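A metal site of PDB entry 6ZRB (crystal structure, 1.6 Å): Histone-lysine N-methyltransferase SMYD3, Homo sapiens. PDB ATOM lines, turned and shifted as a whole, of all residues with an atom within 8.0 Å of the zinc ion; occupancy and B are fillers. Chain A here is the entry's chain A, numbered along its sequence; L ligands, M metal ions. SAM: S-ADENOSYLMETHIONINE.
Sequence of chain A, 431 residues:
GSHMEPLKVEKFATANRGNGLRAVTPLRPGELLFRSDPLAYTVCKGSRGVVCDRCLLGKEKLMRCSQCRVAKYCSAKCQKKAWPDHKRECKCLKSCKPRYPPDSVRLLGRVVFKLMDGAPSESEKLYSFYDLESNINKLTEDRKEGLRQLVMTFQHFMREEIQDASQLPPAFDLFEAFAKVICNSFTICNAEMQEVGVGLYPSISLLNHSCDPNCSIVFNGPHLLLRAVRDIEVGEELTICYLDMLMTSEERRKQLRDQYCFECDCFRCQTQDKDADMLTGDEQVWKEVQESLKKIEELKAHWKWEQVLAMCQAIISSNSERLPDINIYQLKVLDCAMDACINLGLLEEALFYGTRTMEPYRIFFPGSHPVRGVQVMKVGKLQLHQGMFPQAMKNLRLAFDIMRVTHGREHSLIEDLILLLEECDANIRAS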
ATOM      1  N   HIS A 209      17.288  17.726  -7.925  1.00  0.00           N
ATOM      2  CA  HIS A 209      18.089  17.001  -6.915  1.00  0.00           C
ATOM      3  C   HIS A 209      19.284  17.815  -6.449  1.00  0.00           C
ATOM      4  O   HIS A 209      19.956  18.450  -7.276  1.00  0.00           O
ATOM      5  CB  HIS A 209      18.585  15.700  -7.525  1.00  0.00           C
ATOM      6  CG  HIS A 209      19.629  15.045  -6.693  1.00  0.00           C
ATOM      7  ND1 HIS A 209      19.316  14.246  -5.602  1.00  0.00           N
ATOM      8  CD2 HIS A 209      20.977  15.120  -6.762  1.00  0.00           C
ATOM      9  CE1 HIS A 209      20.440  13.839  -5.041  1.00  0.00           C
ATOM     10  NE2 HIS A 209      21.484  14.356  -5.754  1.00  0.00           N
ATOM     11  N   SER A 210      19.614  17.664  -5.175  1.00  0.00           N
ATOM     12  CA  SER A 210      20.946  18.019  -4.636  1.00  0.00           C
ATOM     13  C   SER A 210      21.351  16.974  -3.607  1.00  0.00           C
ATOM     14  O   SER A 210      20.474  16.520  -2.863  1.00  0.00           O
ATOM     15  CB  SER A 210      20.908  19.367  -4.022  1.00  0.00           C
ATOM     16  OG  SER A 210      22.153  19.638  -3.393  1.00  0.00           O
ATOM     17  N   CYS A 211      22.643  16.663  -3.535  1.00  0.00           N
ATOM     18  CA  CYS A 211      23.183  15.783  -2.476  1.00  0.00           C
ATOM     19  C   CYS A 211      23.316  16.565  -1.159  1.00  0.00           C
ATOM     20  O   CYS A 211      23.651  15.944  -0.143  1.00  0.00           O
ATOM     21  CB  CYS A 211      24.509  15.156  -2.882  1.00  0.00           C
ATOM     22  SG  CYS A 211      24.434  14.291  -4.469  1.00  0.00           S
ATOM     23  N   ASP A 212      23.039  17.873  -1.177  1.00  0.00           N
ATOM     24  CA  ASP A 212      22.989  18.734   0.019  1.00  0.00           C
ATOM     25  C   ASP A 212      21.834  19.720  -0.156  1.00  0.00           C
ATOM     26  O   ASP A 212      22.030  20.887  -0.469  1.00  0.00           O
ATOM     27  CB  ASP A 212      24.323  19.414   0.247  1.00  0.00           C
ATOM     28  CG  ASP A 212      24.327  20.320   1.463  1.00  0.00           C
ATOM     29  OD1 ASP A 212      23.410  20.225   2.316  1.00  0.00           O
ATOM     30  OD2 ASP A 212      25.280  21.097   1.557  1.00  0.00           O
ATOM     31  N   CYS A 241      16.954  15.883  -1.910  1.00  0.00           N
ATOM     32  CA  CYS A 241      17.845  14.748  -2.197  1.00  0.00           C
ATOM     33  C   CYS A 241      16.987  13.550  -2.649  1.00  0.00           C
ATOM     34  O   CYS A 241      16.178  13.062  -1.873  1.00  0.00           O
ATOM     35  CB  CYS A 241      18.708  14.415  -0.998  1.00  0.00           C
ATOM     36  SG  CYS A 241      19.979  13.232  -1.472  1.00  0.00           S
ATOM     37  N   LEU A 243      17.943  10.690  -3.087  1.00  0.00           N
ATOM     38  CA  LEU A 243      18.678   9.457  -2.736  1.00  0.00           C
ATOM     39  C   LEU A 243      18.799   9.289  -1.224  1.00  0.00           C
ATOM     40  O   LEU A 243      18.864  10.280  -0.478  1.00  0.00           O
ATOM     41  CB  LEU A 243      20.081   9.533  -3.324  1.00  0.00           C
ATOM     42  CG  LEU A 243      20.155   9.655  -4.834  1.00  0.00           C
ATOM     43  CD1 LEU A 243      21.615   9.677  -5.252  1.00  0.00           C
ATOM     44  CD2 LEU A 243      19.403   8.518  -5.505  1.00  0.00           C
ATOM     45  N   SER A 249      29.647   8.785  -3.239  1.00  0.00           N
ATOM     46  CA  SER A 249      29.519   9.551  -4.514  1.00  0.00           C
ATOM     47  C   SER A 249      29.481   8.577  -5.700  1.00  0.00           C
ATOM     48  O   SER A 249      28.741   8.871  -6.668  1.00  0.00           O
ATOM     49  CB  SER A 249      30.610  10.584  -4.650  1.00  0.00           C
ATOM     50  OG  SER A 249      31.871   9.971  -4.736  1.00  0.00           O
ATOM     51  N   ARG A 252      25.938   7.165  -5.704  1.00  0.00           N
ATOM     52  CA  ARG A 252      25.012   8.237  -6.136  1.00  0.00           C
ATOM     53  C   ARG A 252      25.156   8.432  -7.646  1.00  0.00           C
ATOM     54  O   ARG A 252      24.124   8.575  -8.336  1.00  0.00           O
ATOM     55  CB  ARG A 252      25.238   9.534  -5.360  1.00  0.00           C
ATOM     56  CG  ARG A 252      25.013   9.388  -3.861  1.00  0.00           C
ATOM     57  CD  ARG A 252      24.830  10.706  -3.149  1.00  0.00           C
ATOM     58  NE  ARG A 252      25.881  11.679  -3.395  1.00  0.00           N
ATOM     59  CZ  ARG A 252      27.030  11.738  -2.725  1.00  0.00           C
ATOM     60  NH1 ARG A 252      27.307  10.845  -1.789  1.00  0.00           N
ATOM     61  NH2 ARG A 252      27.928  12.646  -3.032  1.00  0.00           N
ATOM     62  N   ARG A 253      26.383   8.452  -8.156  1.00  0.00           N
ATOM     63  CA  ARG A 253      26.597   8.641  -9.615  1.00  0.00           C
ATOM     64  C   ARG A 253      25.844   7.567 -10.396  1.00  0.00           C
ATOM     65  O   ARG A 253      25.149   7.886 -11.394  1.00  0.00           O
ATOM     66  CB  ARG A 253      28.085   8.582  -9.952  1.00  0.00           C
ATOM     67  CG  ARG A 253      28.364   8.694 -11.450  1.00  0.00           C
ATOM     68  CD  ARG A 253      29.857   8.862 -11.728  1.00  0.00           C
ATOM     69  NE  ARG A 253      30.285  10.168 -11.301  1.00  0.00           N
ATOM     70  CZ  ARG A 253      31.072  10.424 -10.245  1.00  0.00           C
ATOM     71  NH1 ARG A 253      31.568   9.425  -9.516  1.00  0.00           N
ATOM     72  NH2 ARG A 253      31.341  11.686  -9.939  1.00  0.00           N
ATOM     73  N   LEU A 256      21.953   8.152 -10.152  1.00  0.00           N
ATOM     74  CA  LEU A 256      21.491   9.389 -10.832  1.00  0.00           C
ATOM     75  C   LEU A 256      21.661   9.227 -12.350  1.00  0.00           C
ATOM     76  O   LEU A 256      20.810   9.730 -13.089  1.00  0.00           O
ATOM     77  CB  LEU A 256      22.223  10.613 -10.271  1.00  0.00           C
ATOM     78  CG  LEU A 256      21.985  10.887  -8.784  1.00  0.00           C
ATOM     79  CD1 LEU A 256      22.850  12.064  -8.332  1.00  0.00           C
ATOM     80  CD2 LEU A 256      20.508  11.151  -8.508  1.00  0.00           C
ATOM     81  N   PHE A 262      21.230  11.992 -15.286  1.00  0.00           N
ATOM     82  CA  PHE A 262      22.099  13.195 -15.164  1.00  0.00           C
ATOM     83  C   PHE A 262      23.357  12.877 -14.372  1.00  0.00           C
ATOM     84  O   PHE A 262      23.433  11.865 -13.647  1.00  0.00           O
ATOM     85  CB  PHE A 262      21.356  14.418 -14.636  1.00  0.00           C
ATOM     86  CG  PHE A 262      21.041  14.380 -13.159  1.00  0.00           C
ATOM     87  CD1 PHE A 262      19.885  13.779 -12.706  1.00  0.00           C
ATOM     88  CD2 PHE A 262      21.905  14.948 -12.234  1.00  0.00           C
ATOM     89  CE1 PHE A 262      19.579  13.747 -11.358  1.00  0.00           C
ATOM     90  CE2 PHE A 262      21.585  14.917 -10.886  1.00  0.00           C
ATOM     91  CZ  PHE A 262      20.428  14.301 -10.443  1.00  0.00           C
ATOM     92  N   GLU A 263      24.316  13.772 -14.568  1.00  0.00           N
ATOM     93  CA  GLU A 263      25.652  13.780 -13.927  1.00  0.00           C
ATOM     94  C   GLU A 263      25.616  14.873 -12.852  1.00  0.00           C
ATOM     95  O   GLU A 263      25.313  16.012 -13.190  1.00  0.00           O
ATOM     96  CB  GLU A 263      26.724  14.081 -14.969  1.00  0.00           C
ATOM     97  CG  GLU A 263      26.527  13.312 -16.277  1.00  0.00           C
ATOM     98  CD  GLU A 263      26.681  11.823 -16.149  1.00  0.00           C
ATOM     99  OE1 GLU A 263      27.120  11.342 -15.063  1.00  0.00           O
ATOM    100  OE2 GLU A 263      26.353  11.131 -17.109  1.00  0.00           O
ATOM    101  N   CYS A 264      25.788  14.523 -11.579  1.00  0.00           N
ATOM    102  CA  CYS A 264      25.601  15.515 -10.495  1.00  0.00           C
ATOM    103  C   CYS A 264      26.864  16.344 -10.358  1.00  0.00           C
ATOM    104  O   CYS A 264      27.947  15.754 -10.176  1.00  0.00           O
ATOM    105  CB  CYS A 264      25.251  14.884  -9.165  1.00  0.00           C
ATOM    106  SG  CYS A 264      24.781  16.150  -7.935  1.00  0.00           S
ATOM    107  N   ASP A 265      26.687  17.658 -10.435  1.00  0.00           N
ATOM    108  CA  ASP A 265      27.749  18.694 -10.401  1.00  0.00           C
ATOM    109  C   ASP A 265      27.913  19.268  -8.992  1.00  0.00           C
ATOM    110  O   ASP A 265      28.644  20.262  -8.891  1.00  0.00           O
ATOM    111  CB  ASP A 265      27.481  19.856 -11.389  1.00  0.00           C
ATOM    112  CG  ASP A 265      26.273  20.764 -11.163  1.00  0.00           C
ATOM    113  OD1 ASP A 265      26.100  21.719 -11.969  1.00  0.00           O
ATOM    114  OD2 ASP A 265      25.472  20.545 -10.209  1.00  0.00           O
ATOM    115  N   CYS A 266      27.207  18.751  -7.976  1.00  0.00           N
ATOM    116  CA  CYS A 266      27.223  19.407  -6.639  1.00  0.00           C
ATOM    117  C   CYS A 266      28.619  19.282  -5.976  1.00  0.00           C
ATOM    118  O   CYS A 266      29.459  18.456  -6.365  1.00  0.00           O
ATOM    119  CB  CYS A 266      26.105  18.883  -5.736  1.00  0.00           C
ATOM    120  SG  CYS A 266      26.528  17.381  -4.805  1.00  0.00           S
ATOM    121  N   PHE A 267      28.895  20.114  -4.978  1.00  0.00           N
ATOM    122  CA  PHE A 267      30.197  20.146  -4.287  1.00  0.00           C
ATOM    123  C   PHE A 267      30.520  18.765  -3.698  1.00  0.00           C
ATOM    124  O   PHE A 267      31.675  18.324  -3.726  1.00  0.00           O
ATOM    125  CB  PHE A 267      30.168  21.154  -3.152  1.00  0.00           C
ATOM    126  CG  PHE A 267      31.315  20.980  -2.181  1.00  0.00           C
ATOM    127  CD1 PHE A 267      32.578  21.438  -2.512  1.00  0.00           C
ATOM    128  CD2 PHE A 267      31.135  20.333  -0.970  1.00  0.00           C
ATOM    129  CE1 PHE A 267      33.641  21.257  -1.623  1.00  0.00           C
ATOM    130  CE2 PHE A 267      32.198  20.153  -0.090  1.00  0.00           C
ATOM    131  CZ  PHE A 267      33.441  20.633  -0.421  1.00  0.00           C
ATOM    132  N   ARG A 268      29.520  18.087  -3.143  1.00  0.00           N
ATOM    133  CA  ARG A 268      29.778  16.782  -2.505  1.00  0.00           C
ATOM    134  C   ARG A 268      30.275  15.777  -3.556  1.00  0.00           C
ATOM    135  O   ARG A 268      31.159  14.957  -3.225  1.00  0.00           O
ATOM    136  CB  ARG A 268      28.538  16.232  -1.783  1.00  0.00           C
ATOM    137  CG  ARG A 268      28.078  17.100  -0.621  1.00  0.00           C
ATOM    138  CD  ARG A 268      27.064  16.389   0.274  1.00  0.00           C
ATOM    139  NE  ARG A 268      27.702  15.193   0.815  1.00  0.00           N
ATOM    140  CZ  ARG A 268      27.156  13.977   0.876  1.00  0.00           C
ATOM    141  NH1 ARG A 268      25.905  13.757   0.496  1.00  0.00           N
ATOM    142  NH2 ARG A 268      27.896  12.971   1.317  1.00  0.00           N
ATOM    143  N   CYS A 269      29.690  15.781  -4.751  1.00  0.00           N
ATOM    144  CA  CYS A 269      30.114  14.831  -5.803  1.00  0.00           C
ATOM    145  C   CYS A 269      31.493  15.214  -6.323  1.00  0.00           C
ATOM    146  O   CYS A 269      32.319  14.326  -6.502  1.00  0.00           O
ATOM    147  CB  CYS A 269      29.049  14.721  -6.872  1.00  0.00           C
ATOM    148  SG  CYS A 269      27.557  13.943  -6.211  1.00  0.00           S
ATOM    149  N   GLN A 270      31.769  16.503  -6.477  1.00  0.00           N
ATOM    150  CA  GLN A 270      33.090  16.955  -6.968  1.00  0.00           C
ATOM    151  C   GLN A 270      34.208  16.521  -6.006  1.00  0.00           C
ATOM    152  O   GLN A 270      35.353  16.342  -6.466  1.00  0.00           O
ATOM    153  CB  GLN A 270      33.081  18.474  -7.145  1.00  0.00           C
ATOM    154  CG  GLN A 270      32.118  18.971  -8.225  1.00  0.00           C
ATOM    155  CD  GLN A 270      32.164  20.471  -8.392  1.00  0.00           C
ATOM    156  OE1 GLN A 270      33.232  21.067  -8.555  1.00  0.00           O
ATOM    157  NE2 GLN A 270      31.005  21.118  -8.305  1.00  0.00           N
HETATM  158  N   SAM L   1      13.902  19.052 -14.211  1.00  0.00           N
HETATM  159  CA  SAM L   1      12.691  18.192 -14.137  1.00  0.00           C
HETATM  160  C   SAM L   1      11.641  18.669 -15.158  1.00  0.00           C
HETATM  161  O   SAM L   1      10.510  18.149 -15.115  1.00  0.00           O
HETATM  162  OXT SAM L   1      12.031  19.469 -16.038  1.00  0.00           O
HETATM  163  CB  SAM L   1      12.126  18.203 -12.722  1.00  0.00           C
HETATM  164  CG  SAM L   1      12.803  17.176 -11.801  1.00  0.00           C
HETATM  165  SD  SAM L   1      12.350  15.496 -12.347  1.00  0.00           S
HETATM  166  CE  SAM L   1      11.743  14.780 -10.819  1.00  0.00           C
HETATM  167  C5' SAM L   1      13.954  14.661 -12.440  1.00  0.00           C
HETATM  168  C4' SAM L   1      14.799  15.031 -13.634  1.00  0.00           C
HETATM  169  O4' SAM L   1      15.249  16.391 -13.507  1.00  0.00           O
HETATM  170  C3' SAM L   1      16.078  14.210 -13.800  1.00  0.00           C
HETATM  171  O3' SAM L   1      15.764  12.971 -14.427  1.00  0.00           O
HETATM  172  C2' SAM L   1      16.893  15.173 -14.657  1.00  0.00           C
HETATM  173  O2' SAM L   1      16.427  15.236 -15.992  1.00  0.00           O
HETATM  174  C1' SAM L   1      16.589  16.493 -13.956  1.00  0.00           C
HETATM  175  N9  SAM L   1      17.450  16.799 -12.810  1.00  0.00           N
HETATM  176  C8  SAM L   1      17.098  16.728 -11.493  1.00  0.00           C
HETATM  177  N7  SAM L   1      18.029  17.155 -10.677  1.00  0.00           N
HETATM  178  C5  SAM L   1      19.081  17.494 -11.529  1.00  0.00           C
HETATM  179  C6  SAM L   1      20.384  17.979 -11.270  1.00  0.00           C
HETATM  180  N6  SAM L   1      20.845  18.263 -10.058  1.00  0.00           N
HETATM  181  N1  SAM L   1      21.168  18.233 -12.355  1.00  0.00           N
HETATM  182  C2  SAM L   1      20.683  17.994 -13.578  1.00  0.00           C
HETATM  183  N3  SAM L   1      19.494  17.513 -13.926  1.00  0.00           N
HETATM  184  C4  SAM L   1      18.728  17.299 -12.841  1.00  0.00           C
HETATM  185 ZN    ZN M   1      25.859  15.511  -5.972  1.00  0.00          ZN
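N of His 209 lies within hydrogen-bond range of N7 of the ligand, 2.9 Å away.
N6 of the ligand lies within hydrogen-bond range of O of His 209, 2.9 Å away.
Of the 19 residues printed, 4 come within 4 Å of the zinc ion.
The zinc ion is bound by the side-chain sulfur (SG) of Cys 266 (2.3 Å), the side-chain sulfur (SG) of Cys 269 (2.3 Å), the side-chain sulfur (SG) of Cys 264 (2.3 Å) and the side-chain sulfur (SG) of Cys 211 (2.4 Å).
The zinc ion has four donor atoms within binding distance.
N of Arg 268 sits close to SG of Cys 266, at 3.5 Å.
SG of Cys 269 sits close to NH2 of Arg 252 (3.5 Å).
N of Cys 211 is in hydrogen-bond range of NE2 of His 209.
SG of Cys 211 lies close to NE of Arg 252 (3.2 Å).
The guanidinium group of Arg 268 is in hydrogen-bond range of the backbone carbonyl oxygen of Cys 211 (3.2 Å).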
